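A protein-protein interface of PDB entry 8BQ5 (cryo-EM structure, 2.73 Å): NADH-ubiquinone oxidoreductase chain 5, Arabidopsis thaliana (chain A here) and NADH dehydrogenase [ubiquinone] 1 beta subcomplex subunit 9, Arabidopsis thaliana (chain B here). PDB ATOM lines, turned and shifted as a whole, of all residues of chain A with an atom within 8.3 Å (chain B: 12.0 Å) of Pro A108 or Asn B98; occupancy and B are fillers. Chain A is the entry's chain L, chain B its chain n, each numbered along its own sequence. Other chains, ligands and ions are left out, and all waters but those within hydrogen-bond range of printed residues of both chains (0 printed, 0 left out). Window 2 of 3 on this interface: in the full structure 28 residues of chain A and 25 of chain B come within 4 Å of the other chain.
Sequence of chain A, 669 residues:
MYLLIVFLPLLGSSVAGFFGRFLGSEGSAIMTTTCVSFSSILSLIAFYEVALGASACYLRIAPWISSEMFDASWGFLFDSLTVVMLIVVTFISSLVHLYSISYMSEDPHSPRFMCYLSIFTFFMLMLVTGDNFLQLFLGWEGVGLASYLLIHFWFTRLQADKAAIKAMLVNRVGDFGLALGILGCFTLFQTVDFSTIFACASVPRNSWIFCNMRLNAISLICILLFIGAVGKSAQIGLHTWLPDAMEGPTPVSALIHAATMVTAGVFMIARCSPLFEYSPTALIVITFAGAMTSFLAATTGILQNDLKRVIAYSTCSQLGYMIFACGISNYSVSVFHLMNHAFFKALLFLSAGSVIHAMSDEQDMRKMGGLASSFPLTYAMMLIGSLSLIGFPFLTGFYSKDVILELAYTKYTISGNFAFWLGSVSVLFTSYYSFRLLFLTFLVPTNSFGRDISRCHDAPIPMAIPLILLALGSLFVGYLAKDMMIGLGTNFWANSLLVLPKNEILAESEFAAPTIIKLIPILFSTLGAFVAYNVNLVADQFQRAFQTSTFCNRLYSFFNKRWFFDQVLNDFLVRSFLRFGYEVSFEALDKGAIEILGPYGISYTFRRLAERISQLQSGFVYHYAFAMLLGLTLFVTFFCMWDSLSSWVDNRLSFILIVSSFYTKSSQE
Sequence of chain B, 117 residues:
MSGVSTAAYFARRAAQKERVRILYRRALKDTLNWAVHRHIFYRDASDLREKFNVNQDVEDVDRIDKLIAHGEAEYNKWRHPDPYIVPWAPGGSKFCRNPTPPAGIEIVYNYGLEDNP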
ATOM      1  N   GLY A  24     -34.747   1.625  24.804  1.00  0.00           N
ATOM      2  CA  GLY A  24     -33.589   1.653  23.934  1.00  0.00           C
ATOM      3  C   GLY A  24     -32.399   2.359  24.571  1.00  0.00           C
ATOM      4  O   GLY A  24     -32.383   2.696  25.751  1.00  0.00           O
ATOM      5  N   SER A  25     -31.384   2.579  23.735  1.00  0.00           N
ATOM      6  CA  SER A  25     -30.178   3.255  24.201  1.00  0.00           C
ATOM      7  C   SER A  25     -30.482   4.677  24.652  1.00  0.00           C
ATOM      8  O   SER A  25     -29.997   5.126  25.696  1.00  0.00           O
ATOM      9  CB  SER A  25     -29.117   3.258  23.101  1.00  0.00           C
ATOM     10  OG  SER A  25     -28.863   1.946  22.634  1.00  0.00           O
ATOM     11  N   MET A 104     -20.314   5.681  25.710  1.00  0.00           N
ATOM     12  CA  MET A 104     -20.891   4.407  25.305  1.00  0.00           C
ATOM     13  C   MET A 104     -21.928   4.569  24.201  1.00  0.00           C
ATOM     14  O   MET A 104     -22.851   3.754  24.101  1.00  0.00           O
ATOM     15  CB  MET A 104     -21.506   3.692  26.510  1.00  0.00           C
ATOM     16  CG  MET A 104     -20.514   3.357  27.615  1.00  0.00           C
ATOM     17  SD  MET A 104     -19.392   2.015  27.179  1.00  0.00           S
ATOM     18  CE  MET A 104     -20.413   0.585  27.528  1.00  0.00           C
ATOM     19  N   SER A 105     -21.797   5.612  23.377  1.00  0.00           N
ATOM     20  CA  SER A 105     -22.772   5.853  22.318  1.00  0.00           C
ATOM     21  C   SER A 105     -22.787   4.726  21.296  1.00  0.00           C
ATOM     22  O   SER A 105     -23.861   4.320  20.837  1.00  0.00           O
ATOM     23  CB  SER A 105     -22.483   7.188  21.630  1.00  0.00           C
ATOM     24  OG  SER A 105     -21.428   7.067  20.691  1.00  0.00           O
ATOM     25  N   GLU A 106     -21.620   4.210  20.927  1.00  0.00           N
ATOM     26  CA  GLU A 106     -21.525   3.206  19.878  1.00  0.00           C
ATOM     27  C   GLU A 106     -21.518   1.776  20.410  1.00  0.00           C
ATOM     28  O   GLU A 106     -21.359   0.842  19.618  1.00  0.00           O
ATOM     29  CB  GLU A 106     -20.271   3.451  19.033  1.00  0.00           C
ATOM     30  CG  GLU A 106     -19.962   4.926  18.799  1.00  0.00           C
ATOM     31  CD  GLU A 106     -20.707   5.509  17.614  1.00  0.00           C
ATOM     32  OE1 GLU A 106     -20.376   5.150  16.464  1.00  0.00           O
ATOM     33  OE2 GLU A 106     -21.620   6.335  17.831  1.00  0.00           O
ATOM     34  N   ASP A 107     -21.678   1.579  21.717  1.00  0.00           N
ATOM     35  CA  ASP A 107     -21.704   0.229  22.265  1.00  0.00           C
ATOM     36  C   ASP A 107     -23.061  -0.424  22.001  1.00  0.00           C
ATOM     37  O   ASP A 107     -24.098   0.240  22.089  1.00  0.00           O
ATOM     38  CB  ASP A 107     -21.416   0.249  23.767  1.00  0.00           C
ATOM     39  CG  ASP A 107     -21.142  -1.137  24.330  1.00  0.00           C
ATOM     40  OD1 ASP A 107     -22.109  -1.889  24.571  1.00  0.00           O
ATOM     41  OD2 ASP A 107     -19.958  -1.480  24.522  1.00  0.00           O
ATOM     42  N   PRO A 108     -23.086  -1.716  21.665  1.00  0.00           N
ATOM     43  CA  PRO A 108     -24.378  -2.381  21.434  1.00  0.00           C
ATOM     44  C   PRO A 108     -25.258  -2.466  22.670  1.00  0.00           C
ATOM     45  O   PRO A 108     -26.486  -2.473  22.536  1.00  0.00           O
ATOM     46  CB  PRO A 108     -23.978  -3.779  20.938  1.00  0.00           C
ATOM     47  CG  PRO A 108     -22.544  -3.676  20.556  1.00  0.00           C
ATOM     48  CD  PRO A 108     -21.946  -2.612  21.411  1.00  0.00           C
ATOM     49  N   HIS A 109     -24.676  -2.523  23.865  1.00  0.00           N
ATOM     50  CA  HIS A 109     -25.408  -2.853  25.085  1.00  0.00           C
ATOM     51  C   HIS A 109     -25.373  -1.719  26.107  1.00  0.00           C
ATOM     52  O   HIS A 109     -25.157  -1.945  27.299  1.00  0.00           O
ATOM     53  CB  HIS A 109     -24.860  -4.137  25.695  1.00  0.00           C
ATOM     54  CG  HIS A 109     -24.911  -5.309  24.766  1.00  0.00           C
ATOM     55  ND1 HIS A 109     -23.788  -5.830  24.163  1.00  0.00           N
ATOM     56  CD2 HIS A 109     -25.953  -6.055  24.332  1.00  0.00           C
ATOM     57  CE1 HIS A 109     -24.136  -6.849  23.398  1.00  0.00           C
ATOM     58  NE2 HIS A 109     -25.443  -7.007  23.484  1.00  0.00           N
ATOM     59  N   SER A 110     -25.589  -0.488  25.646  1.00  0.00           N
ATOM     60  CA  SER A 110     -25.633   0.650  26.562  1.00  0.00           C
ATOM     61  C   SER A 110     -26.739   0.570  27.612  1.00  0.00           C
ATOM     62  O   SER A 110     -26.458   0.898  28.777  1.00  0.00           O
ATOM     63  CB  SER A 110     -25.749   1.954  25.763  1.00  0.00           C
ATOM     64  OG  SER A 110     -25.005   1.880  24.562  1.00  0.00           O
ATOM     65  N   PRO A 111     -27.988   0.193  27.293  1.00  0.00           N
ATOM     66  CA  PRO A 111     -29.025   0.206  28.342  1.00  0.00           C
ATOM     67  C   PRO A 111     -28.700  -0.675  29.535  1.00  0.00           C
ATOM     68  O   PRO A 111     -29.076  -0.341  30.665  1.00  0.00           O
ATOM     69  CB  PRO A 111     -30.277  -0.285  27.602  1.00  0.00           C
ATOM     70  CG  PRO A 111     -30.026   0.037  26.190  1.00  0.00           C
ATOM     71  CD  PRO A 111     -28.561  -0.171  25.986  1.00  0.00           C
ATOM     72  N   ARG A 112     -28.019  -1.800  29.316  1.00  0.00           N
ATOM     73  CA  ARG A 112     -27.598  -2.629  30.438  1.00  0.00           C
ATOM     74  C   ARG A 112     -26.444  -1.981  31.191  1.00  0.00           C
ATOM     75  O   ARG A 112     -26.345  -2.101  32.417  1.00  0.00           O
ATOM     76  CB  ARG A 112     -27.212  -4.022  29.945  1.00  0.00           C
ATOM     77  CG  ARG A 112     -26.971  -5.025  31.052  1.00  0.00           C
ATOM     78  CD  ARG A 112     -26.622  -6.387  30.487  1.00  0.00           C
ATOM     79  NE  ARG A 112     -25.182  -6.585  30.384  1.00  0.00           N
ATOM     80  CZ  ARG A 112     -24.511  -6.643  29.242  1.00  0.00           C
ATOM     81  NH1 ARG A 112     -25.120  -6.524  28.075  1.00  0.00           N
ATOM     82  NH2 ARG A 112     -23.194  -6.825  29.273  1.00  0.00           N
ATOM     83  N   PHE A 113     -25.558  -1.290  30.471  1.00  0.00           N
ATOM     84  CA  PHE A 113     -24.456  -0.593  31.122  1.00  0.00           C
ATOM     85  C   PHE A 113     -24.969   0.502  32.049  1.00  0.00           C
ATOM     86  O   PHE A 113     -24.511   0.631  33.189  1.00  0.00           O
ATOM     87  CB  PHE A 113     -23.514  -0.007  30.074  1.00  0.00           C
ATOM     88  CG  PHE A 113     -22.325   0.686  30.660  1.00  0.00           C
ATOM     89  CD1 PHE A 113     -21.244  -0.043  31.119  1.00  0.00           C
ATOM     90  CD2 PHE A 113     -22.293   2.065  30.767  1.00  0.00           C
ATOM     91  CE1 PHE A 113     -20.149   0.592  31.663  1.00  0.00           C
ATOM     92  CE2 PHE A 113     -21.202   2.705  31.311  1.00  0.00           C
ATOM     93  CZ  PHE A 113     -20.128   1.968  31.760  1.00  0.00           C
ATOM     94  N   PHE A 153     -18.232  -6.500  31.963  1.00  0.00           N
ATOM     95  CA  PHE A 153     -19.353  -6.064  31.138  1.00  0.00           C
ATOM     96  C   PHE A 153     -19.256  -6.620  29.723  1.00  0.00           C
ATOM     97  O   PHE A 153     -20.263  -7.031  29.136  1.00  0.00           O
ATOM     98  CB  PHE A 153     -19.410  -4.538  31.114  1.00  0.00           C
ATOM     99  CG  PHE A 153     -20.411  -3.985  30.153  1.00  0.00           C
ATOM    100  CD1 PHE A 153     -21.762  -4.016  30.444  1.00  0.00           C
ATOM    101  CD2 PHE A 153     -20.001  -3.434  28.952  1.00  0.00           C
ATOM    102  CE1 PHE A 153     -22.684  -3.506  29.558  1.00  0.00           C
ATOM    103  CE2 PHE A 153     -20.921  -2.925  28.062  1.00  0.00           C
ATOM    104  CZ  PHE A 153     -22.263  -2.960  28.366  1.00  0.00           C
ATOM    105  N   TRP A 154     -18.049  -6.637  29.156  1.00  0.00           N
ATOM    106  CA  TRP A 154     -17.804  -7.313  27.883  1.00  0.00           C
ATOM    107  C   TRP A 154     -17.533  -8.783  28.183  1.00  0.00           C
ATOM    108  O   TRP A 154     -16.393  -9.245  28.267  1.00  0.00           O
ATOM    109  CB  TRP A 154     -16.652  -6.655  27.138  1.00  0.00           C
ATOM    110  CG  TRP A 154     -16.995  -5.286  26.663  1.00  0.00           C
ATOM    111  CD1 TRP A 154     -18.097  -4.923  25.944  1.00  0.00           C
ATOM    112  CD2 TRP A 154     -16.242  -4.089  26.877  1.00  0.00           C
ATOM    113  NE1 TRP A 154     -18.072  -3.574  25.692  1.00  0.00           N
ATOM    114  CE2 TRP A 154     -16.943  -3.039  26.254  1.00  0.00           C
ATOM    115  CE3 TRP A 154     -15.039  -3.804  27.530  1.00  0.00           C
ATOM    116  CZ2 TRP A 154     -16.484  -1.725  26.267  1.00  0.00           C
ATOM    117  CZ3 TRP A 154     -14.584  -2.500  27.540  1.00  0.00           C
ATOM    118  CH2 TRP A 154     -15.305  -1.476  26.914  1.00  0.00           C
ATOM    119  N   PHE A 155     -18.626  -9.532  28.340  1.00  0.00           N
ATOM    120  CA  PHE A 155     -18.547 -10.885  28.873  1.00  0.00           C
ATOM    121  C   PHE A 155     -17.864 -11.863  27.925  1.00  0.00           C
ATOM    122  O   PHE A 155     -17.561 -12.988  28.331  1.00  0.00           O
ATOM    123  CB  PHE A 155     -19.953 -11.374  29.230  1.00  0.00           C
ATOM    124  CG  PHE A 155     -20.976 -11.111  28.162  1.00  0.00           C
ATOM    125  CD1 PHE A 155     -20.987 -11.850  26.992  1.00  0.00           C
ATOM    126  CD2 PHE A 155     -21.925 -10.118  28.329  1.00  0.00           C
ATOM    127  CE1 PHE A 155     -21.925 -11.606  26.013  1.00  0.00           C
ATOM    128  CE2 PHE A 155     -22.868  -9.872  27.350  1.00  0.00           C
ATOM    129  CZ  PHE A 155     -22.867 -10.618  26.192  1.00  0.00           C
ATOM    130  N   THR A 156     -17.626 -11.469  26.676  1.00  0.00           N
ATOM    131  CA  THR A 156     -16.931 -12.331  25.728  1.00  0.00           C
ATOM    132  C   THR A 156     -15.423 -12.328  25.921  1.00  0.00           C
ATOM    133  O   THR A 156     -14.746 -13.229  25.417  1.00  0.00           O
ATOM    134  CB  THR A 156     -17.252 -11.905  24.296  1.00  0.00           C
ATOM    135  OG1 THR A 156     -17.264 -10.475  24.219  1.00  0.00           O
ATOM    136  CG2 THR A 156     -18.611 -12.437  23.880  1.00  0.00           C
ATOM    137  N   ARG A 157     -14.887 -11.347  26.636  1.00  0.00           N
ATOM    138  CA  ARG A 157     -13.452 -11.208  26.818  1.00  0.00           C
ATOM    139  C   ARG A 157     -13.006 -12.069  27.993  1.00  0.00           C
ATOM    140  O   ARG A 157     -13.506 -11.909  29.111  1.00  0.00           O
ATOM    141  CB  ARG A 157     -13.091  -9.744  27.046  1.00  0.00           C
ATOM    142  CG  ARG A 157     -11.675  -9.404  26.686  1.00  0.00           C
ATOM    143  CD  ARG A 157     -11.483  -7.907  26.630  1.00  0.00           C
ATOM    144  NE  ARG A 157     -10.281  -7.501  27.345  1.00  0.00           N
ATOM    145  CZ  ARG A 157      -9.054  -7.593  26.854  1.00  0.00           C
ATOM    146  NH1 ARG A 157      -8.828  -8.076  25.644  1.00  0.00           N
ATOM    147  NH2 ARG A 157      -8.027  -7.191  27.597  1.00  0.00           N
ATOM    148  N   PRO B  87      -4.389  -3.233  19.677  1.00  0.00           N
ATOM    149  CA  PRO B  87      -5.535  -3.512  20.564  1.00  0.00           C
ATOM    150  C   PRO B  87      -6.421  -4.673  20.138  1.00  0.00           C
ATOM    151  O   PRO B  87      -6.872  -5.431  21.005  1.00  0.00           O
ATOM    152  CB  PRO B  87      -6.310  -2.188  20.544  1.00  0.00           C
ATOM    153  CG  PRO B  87      -5.266  -1.160  20.297  1.00  0.00           C
ATOM    154  CD  PRO B  87      -4.264  -1.795  19.378  1.00  0.00           C
ATOM    155  N   TRP B  88      -6.692  -4.844  18.849  1.00  0.00           N
ATOM    156  CA  TRP B  88      -7.564  -5.922  18.407  1.00  0.00           C
ATOM    157  C   TRP B  88      -6.814  -7.221  18.138  1.00  0.00           C
ATOM    158  O   TRP B  88      -7.450  -8.239  17.849  1.00  0.00           O
ATOM    159  CB  TRP B  88      -8.340  -5.497  17.158  1.00  0.00           C
ATOM    160  CG  TRP B  88      -7.486  -4.853  16.126  1.00  0.00           C
ATOM    161  CD1 TRP B  88      -7.339  -3.517  15.901  1.00  0.00           C
ATOM    162  CD2 TRP B  88      -6.658  -5.516  15.166  1.00  0.00           C
ATOM    163  NE1 TRP B  88      -6.465  -3.306  14.865  1.00  0.00           N
ATOM    164  CE2 TRP B  88      -6.033  -4.518  14.395  1.00  0.00           C
ATOM    165  CE3 TRP B  88      -6.381  -6.858  14.886  1.00  0.00           C
ATOM    166  CZ2 TRP B  88      -5.150  -4.818  13.362  1.00  0.00           C
ATOM    167  CZ3 TRP B  88      -5.504  -7.154  13.860  1.00  0.00           C
ATOM    168  CH2 TRP B  88      -4.899  -6.139  13.111  1.00  0.00           C
ATOM    169  N   GLY B  92      -4.496  -8.123  23.069  1.00  0.00           N
ATOM    170  CA  GLY B  92      -4.691  -6.692  23.120  1.00  0.00           C
ATOM    171  C   GLY B  92      -5.861  -6.298  23.998  1.00  0.00           C
ATOM    172  O   GLY B  92      -6.677  -7.122  24.408  1.00  0.00           O
ATOM    173  N   SER B  93      -5.943  -4.995  24.279  1.00  0.00           N
ATOM    174  CA  SER B  93      -6.966  -4.498  25.193  1.00  0.00           C
ATOM    175  C   SER B  93      -8.350  -4.501  24.557  1.00  0.00           C
ATOM    176  O   SER B  93      -9.357  -4.479  25.273  1.00  0.00           O
ATOM    177  CB  SER B  93      -6.609  -3.090  25.665  1.00  0.00           C
ATOM    178  OG  SER B  93      -6.569  -2.181  24.580  1.00  0.00           O
ATOM    179  N   LYS B  94      -8.426  -4.515  23.229  1.00  0.00           N
ATOM    180  CA  LYS B  94      -9.699  -4.556  22.526  1.00  0.00           C
ATOM    181  C   LYS B  94     -10.053  -5.952  22.028  1.00  0.00           C
ATOM    182  O   LYS B  94     -11.066  -6.113  21.341  1.00  0.00           O
ATOM    183  CB  LYS B  94      -9.681  -3.570  21.351  1.00  0.00           C
ATOM    184  CG  LYS B  94     -11.052  -3.036  20.961  1.00  0.00           C
ATOM    185  CD  LYS B  94     -11.121  -2.712  19.478  1.00  0.00           C
ATOM    186  CE  LYS B  94     -11.417  -1.242  19.243  1.00  0.00           C
ATOM    187  NZ  LYS B  94     -11.358  -0.881  17.800  1.00  0.00           N
ATOM    188  N   PHE B  95      -9.253  -6.963  22.361  1.00  0.00           N
ATOM    189  CA  PHE B  95      -9.486  -8.305  21.843  1.00  0.00           C
ATOM    190  C   PHE B  95     -10.758  -8.905  22.433  1.00  0.00           C
ATOM    191  O   PHE B  95     -11.019  -8.775  23.632  1.00  0.00           O
ATOM    192  CB  PHE B  95      -8.291  -9.208  22.145  1.00  0.00           C
ATOM    193  CG  PHE B  95      -8.277 -10.476  21.340  1.00  0.00           C
ATOM    194  CD1 PHE B  95      -8.507 -10.447  19.976  1.00  0.00           C
ATOM    195  CD2 PHE B  95      -8.041 -11.697  21.949  1.00  0.00           C
ATOM    196  CE1 PHE B  95      -8.499 -11.611  19.231  1.00  0.00           C
ATOM    197  CE2 PHE B  95      -8.032 -12.867  21.208  1.00  0.00           C
ATOM    198  CZ  PHE B  95      -8.262 -12.823  19.848  1.00  0.00           C
ATOM    199  N   CYS B  96     -11.546  -9.564  21.580  1.00  0.00           N
ATOM    200  CA  CYS B  96     -12.781 -10.245  21.970  1.00  0.00           C
ATOM    201  C   CYS B  96     -13.818  -9.289  22.555  1.00  0.00           C
ATOM    202  O   CYS B  96     -14.703  -9.711  23.303  1.00  0.00           O
ATOM    203  CB  CYS B  96     -12.509 -11.389  22.954  1.00  0.00           C
ATOM    204  SG  CYS B  96     -11.331 -12.630  22.379  1.00  0.00           S
ATOM    205  N   ARG B  97     -13.729  -8.003  22.227  1.00  0.00           N
ATOM    206  CA  ARG B  97     -14.707  -7.026  22.683  1.00  0.00           C
ATOM    207  C   ARG B  97     -15.741  -6.785  21.592  1.00  0.00           C
ATOM    208  O   ARG B  97     -15.394  -6.359  20.486  1.00  0.00           O
ATOM    209  CB  ARG B  97     -14.037  -5.709  23.067  1.00  0.00           C
ATOM    210  CG  ARG B  97     -15.000  -4.726  23.699  1.00  0.00           C
ATOM    211  CD  ARG B  97     -14.521  -3.296  23.578  1.00  0.00           C
ATOM    212  NE  ARG B  97     -13.301  -3.052  24.335  1.00  0.00           N
ATOM    213  CZ  ARG B  97     -12.724  -1.863  24.453  1.00  0.00           C
ATOM    214  NH1 ARG B  97     -13.230  -0.790  23.870  1.00  0.00           N
ATOM    215  NH2 ARG B  97     -11.617  -1.749  25.180  1.00  0.00           N
ATOM    216  N   ASN B  98     -17.010  -7.037  21.921  1.00  0.00           N
ATOM    217  CA  ASN B  98     -18.124  -6.995  20.980  1.00  0.00           C
ATOM    218  C   ASN B  98     -17.782  -7.721  19.684  1.00  0.00           C
ATOM    219  O   ASN B  98     -17.834  -7.115  18.606  1.00  0.00           O
ATOM    220  CB  ASN B  98     -18.528  -5.549  20.682  1.00  0.00           C
ATOM    221  CG  ASN B  98     -18.969  -4.802  21.922  1.00  0.00           C
ATOM    222  OD1 ASN B  98     -19.778  -5.300  22.705  1.00  0.00           O
ATOM    223  ND2 ASN B  98     -18.442  -3.600  22.107  1.00  0.00           N
ATOM    224  N   PRO B  99     -17.422  -9.002  19.738  1.00  0.00           N
ATOM    225  CA  PRO B  99     -17.114  -9.720  18.501  1.00  0.00           C
ATOM    226  C   PRO B  99     -18.382 -10.036  17.727  1.00  0.00           C
ATOM    227  O   PRO B  99     -19.483 -10.072  18.279  1.00  0.00           O
ATOM    228  CB  PRO B  99     -16.430 -10.995  18.997  1.00  0.00           C
ATOM    229  CG  PRO B  99     -17.046 -11.239  20.322  1.00  0.00           C
ATOM    230  CD  PRO B  99     -17.364  -9.891  20.913  1.00  0.00           C
ATOM    231  N   THR B 100     -18.215 -10.255  16.429  1.00  0.00           N
ATOM    232  CA  THR B 100     -19.361 -10.563  15.588  1.00  0.00           C
ATOM    233  C   THR B 100     -19.942 -11.921  15.977  1.00  0.00           C
ATOM    234  O   THR B 100     -19.191 -12.872  16.224  1.00  0.00           O
ATOM    235  CB  THR B 100     -18.966 -10.554  14.109  1.00  0.00           C
ATOM    236  OG1 THR B 100     -19.998 -11.170  13.330  1.00  0.00           O
ATOM    237  CG2 THR B 100     -17.659 -11.296  13.895  1.00  0.00           C
ATOM    238  N   PRO B 101     -21.269 -12.041  16.062  1.00  0.00           N
ATOM    239  CA  PRO B 101     -21.861 -13.320  16.451  1.00  0.00           C
ATOM    240  C   PRO B 101     -21.537 -14.399  15.434  1.00  0.00           C
ATOM    241  O   PRO B 101     -21.488 -14.134  14.220  1.00  0.00           O
ATOM    242  CB  PRO B 101     -23.370 -13.018  16.483  1.00  0.00           C
ATOM    243  CG  PRO B 101     -23.495 -11.541  16.451  1.00  0.00           C
ATOM    244  CD  PRO B 101     -22.278 -11.011  15.779  1.00  0.00           C
ATOM    245  N   PRO B 102     -21.312 -15.633  15.879  1.00  0.00           N
ATOM    246  CA  PRO B 102     -21.028 -16.712  14.930  1.00  0.00           C
ATOM    247  C   PRO B 102     -22.248 -17.055  14.092  1.00  0.00           C
ATOM    248  O   PRO B 102     -23.395 -16.885  14.515  1.00  0.00           O
ATOM    249  CB  PRO B 102     -20.633 -17.878  15.841  1.00  0.00           C
ATOM    250  CG  PRO B 102     -21.459 -17.635  17.063  1.00  0.00           C
ATOM    251  CD  PRO B 102     -21.359 -16.138  17.262  1.00  0.00           C
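The side-chain carboxylate (OD2) of Asp A107 lies within hydrogen-bond range of the indole nitrogen (NE1) of Trp A154 (3.1 Å).
OD1 of Asp A107 lies within hydrogen-bond range of N of His A109 (2.7 Å).
O of Pro B87 sits at hydrogen-bond distance from N of Ser B93, at 3.4 Å.
The backbone carbonyl oxygen (O) of Asp A107 is in hydrogen-bond range of the side-chain hydroxyl (OG) of Ser A110, at 3.1 Å.
O of Pro B87 lies within hydrogen-bond range of N of Phe B95 (3.1 Å).
Of the 17 printed residues of chain A, 5 touch a printed residue of chain B.
Of the 13 printed residues of chain B, 7 touch a printed residue of chain A.
Among the printed residues, 10 pairs touch across the chains.
Among the printed residues, no Asp or Glu carboxylate lies within 4 Å of a Lys or Arg side-chain nitrogen of the other chain.
Among the printed residues, pairs that only touch across the chains: Asp A107 with Asn B98 (3.6 Å), Pro A108 with Asn B98 (3.7 Å), Trp A154 with Arg B97 (3.5 Å), Trp A154 with Asn B98 (3.6 Å), Thr A156 with Pro B99 (3.4 Å), Arg A157 with Ser B93 (3.5 Å) and Arg A157 with Cys B96 (3.7 Å).
Asn B98 touches just these residues of chain A: Asp A107, Pro A108 and Trp A154.
Printed residues of chain B within 4 Å of Asp A107: Asn B98.
No residue of chain B comes within 4 Å of Ser A110.
Trp A154 touches just these residues of chain B: Arg B97 (3.5 Å) and Asn B98 (3.6 Å).
Thr A156 touches just these residues of chain B: Cys B96 (2.8 Å) and Pro B99 (3.4 Å).
Of chain A, only Thr A156 (3.4 Å) comes within 4 Å of Pro B99.
Printed residues of chain A within 4 Å of Arg B97: Trp A154 (3.5 Å).
Of the printed residues of chain A, Ser B93 touches Arg A157.
Printed residues of chain B within 4 Å of Arg A157: Gly B92, Ser B93, Phe B95 and Cys B96.
The nearest residue of chain A that does not touch Asn B98 is Thr A156 (4.1 Å).
The side-chain hydroxyl (OG1) of Thr A156 lies within hydrogen-bond range of the backbone carbonyl oxygen (O) of Cys B96 (2.8 Å).
The guanidinium group (NH1) of Arg A157 lies within hydrogen-bond range of the backbone carbonyl oxygen (O) of Gly B92 (2.7 Å).
The backbone carbonyl oxygen (O) of Phe B95 is in hydrogen-bond range of the guanidinium group (NH1) of Arg A157, 3.1 Å away.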
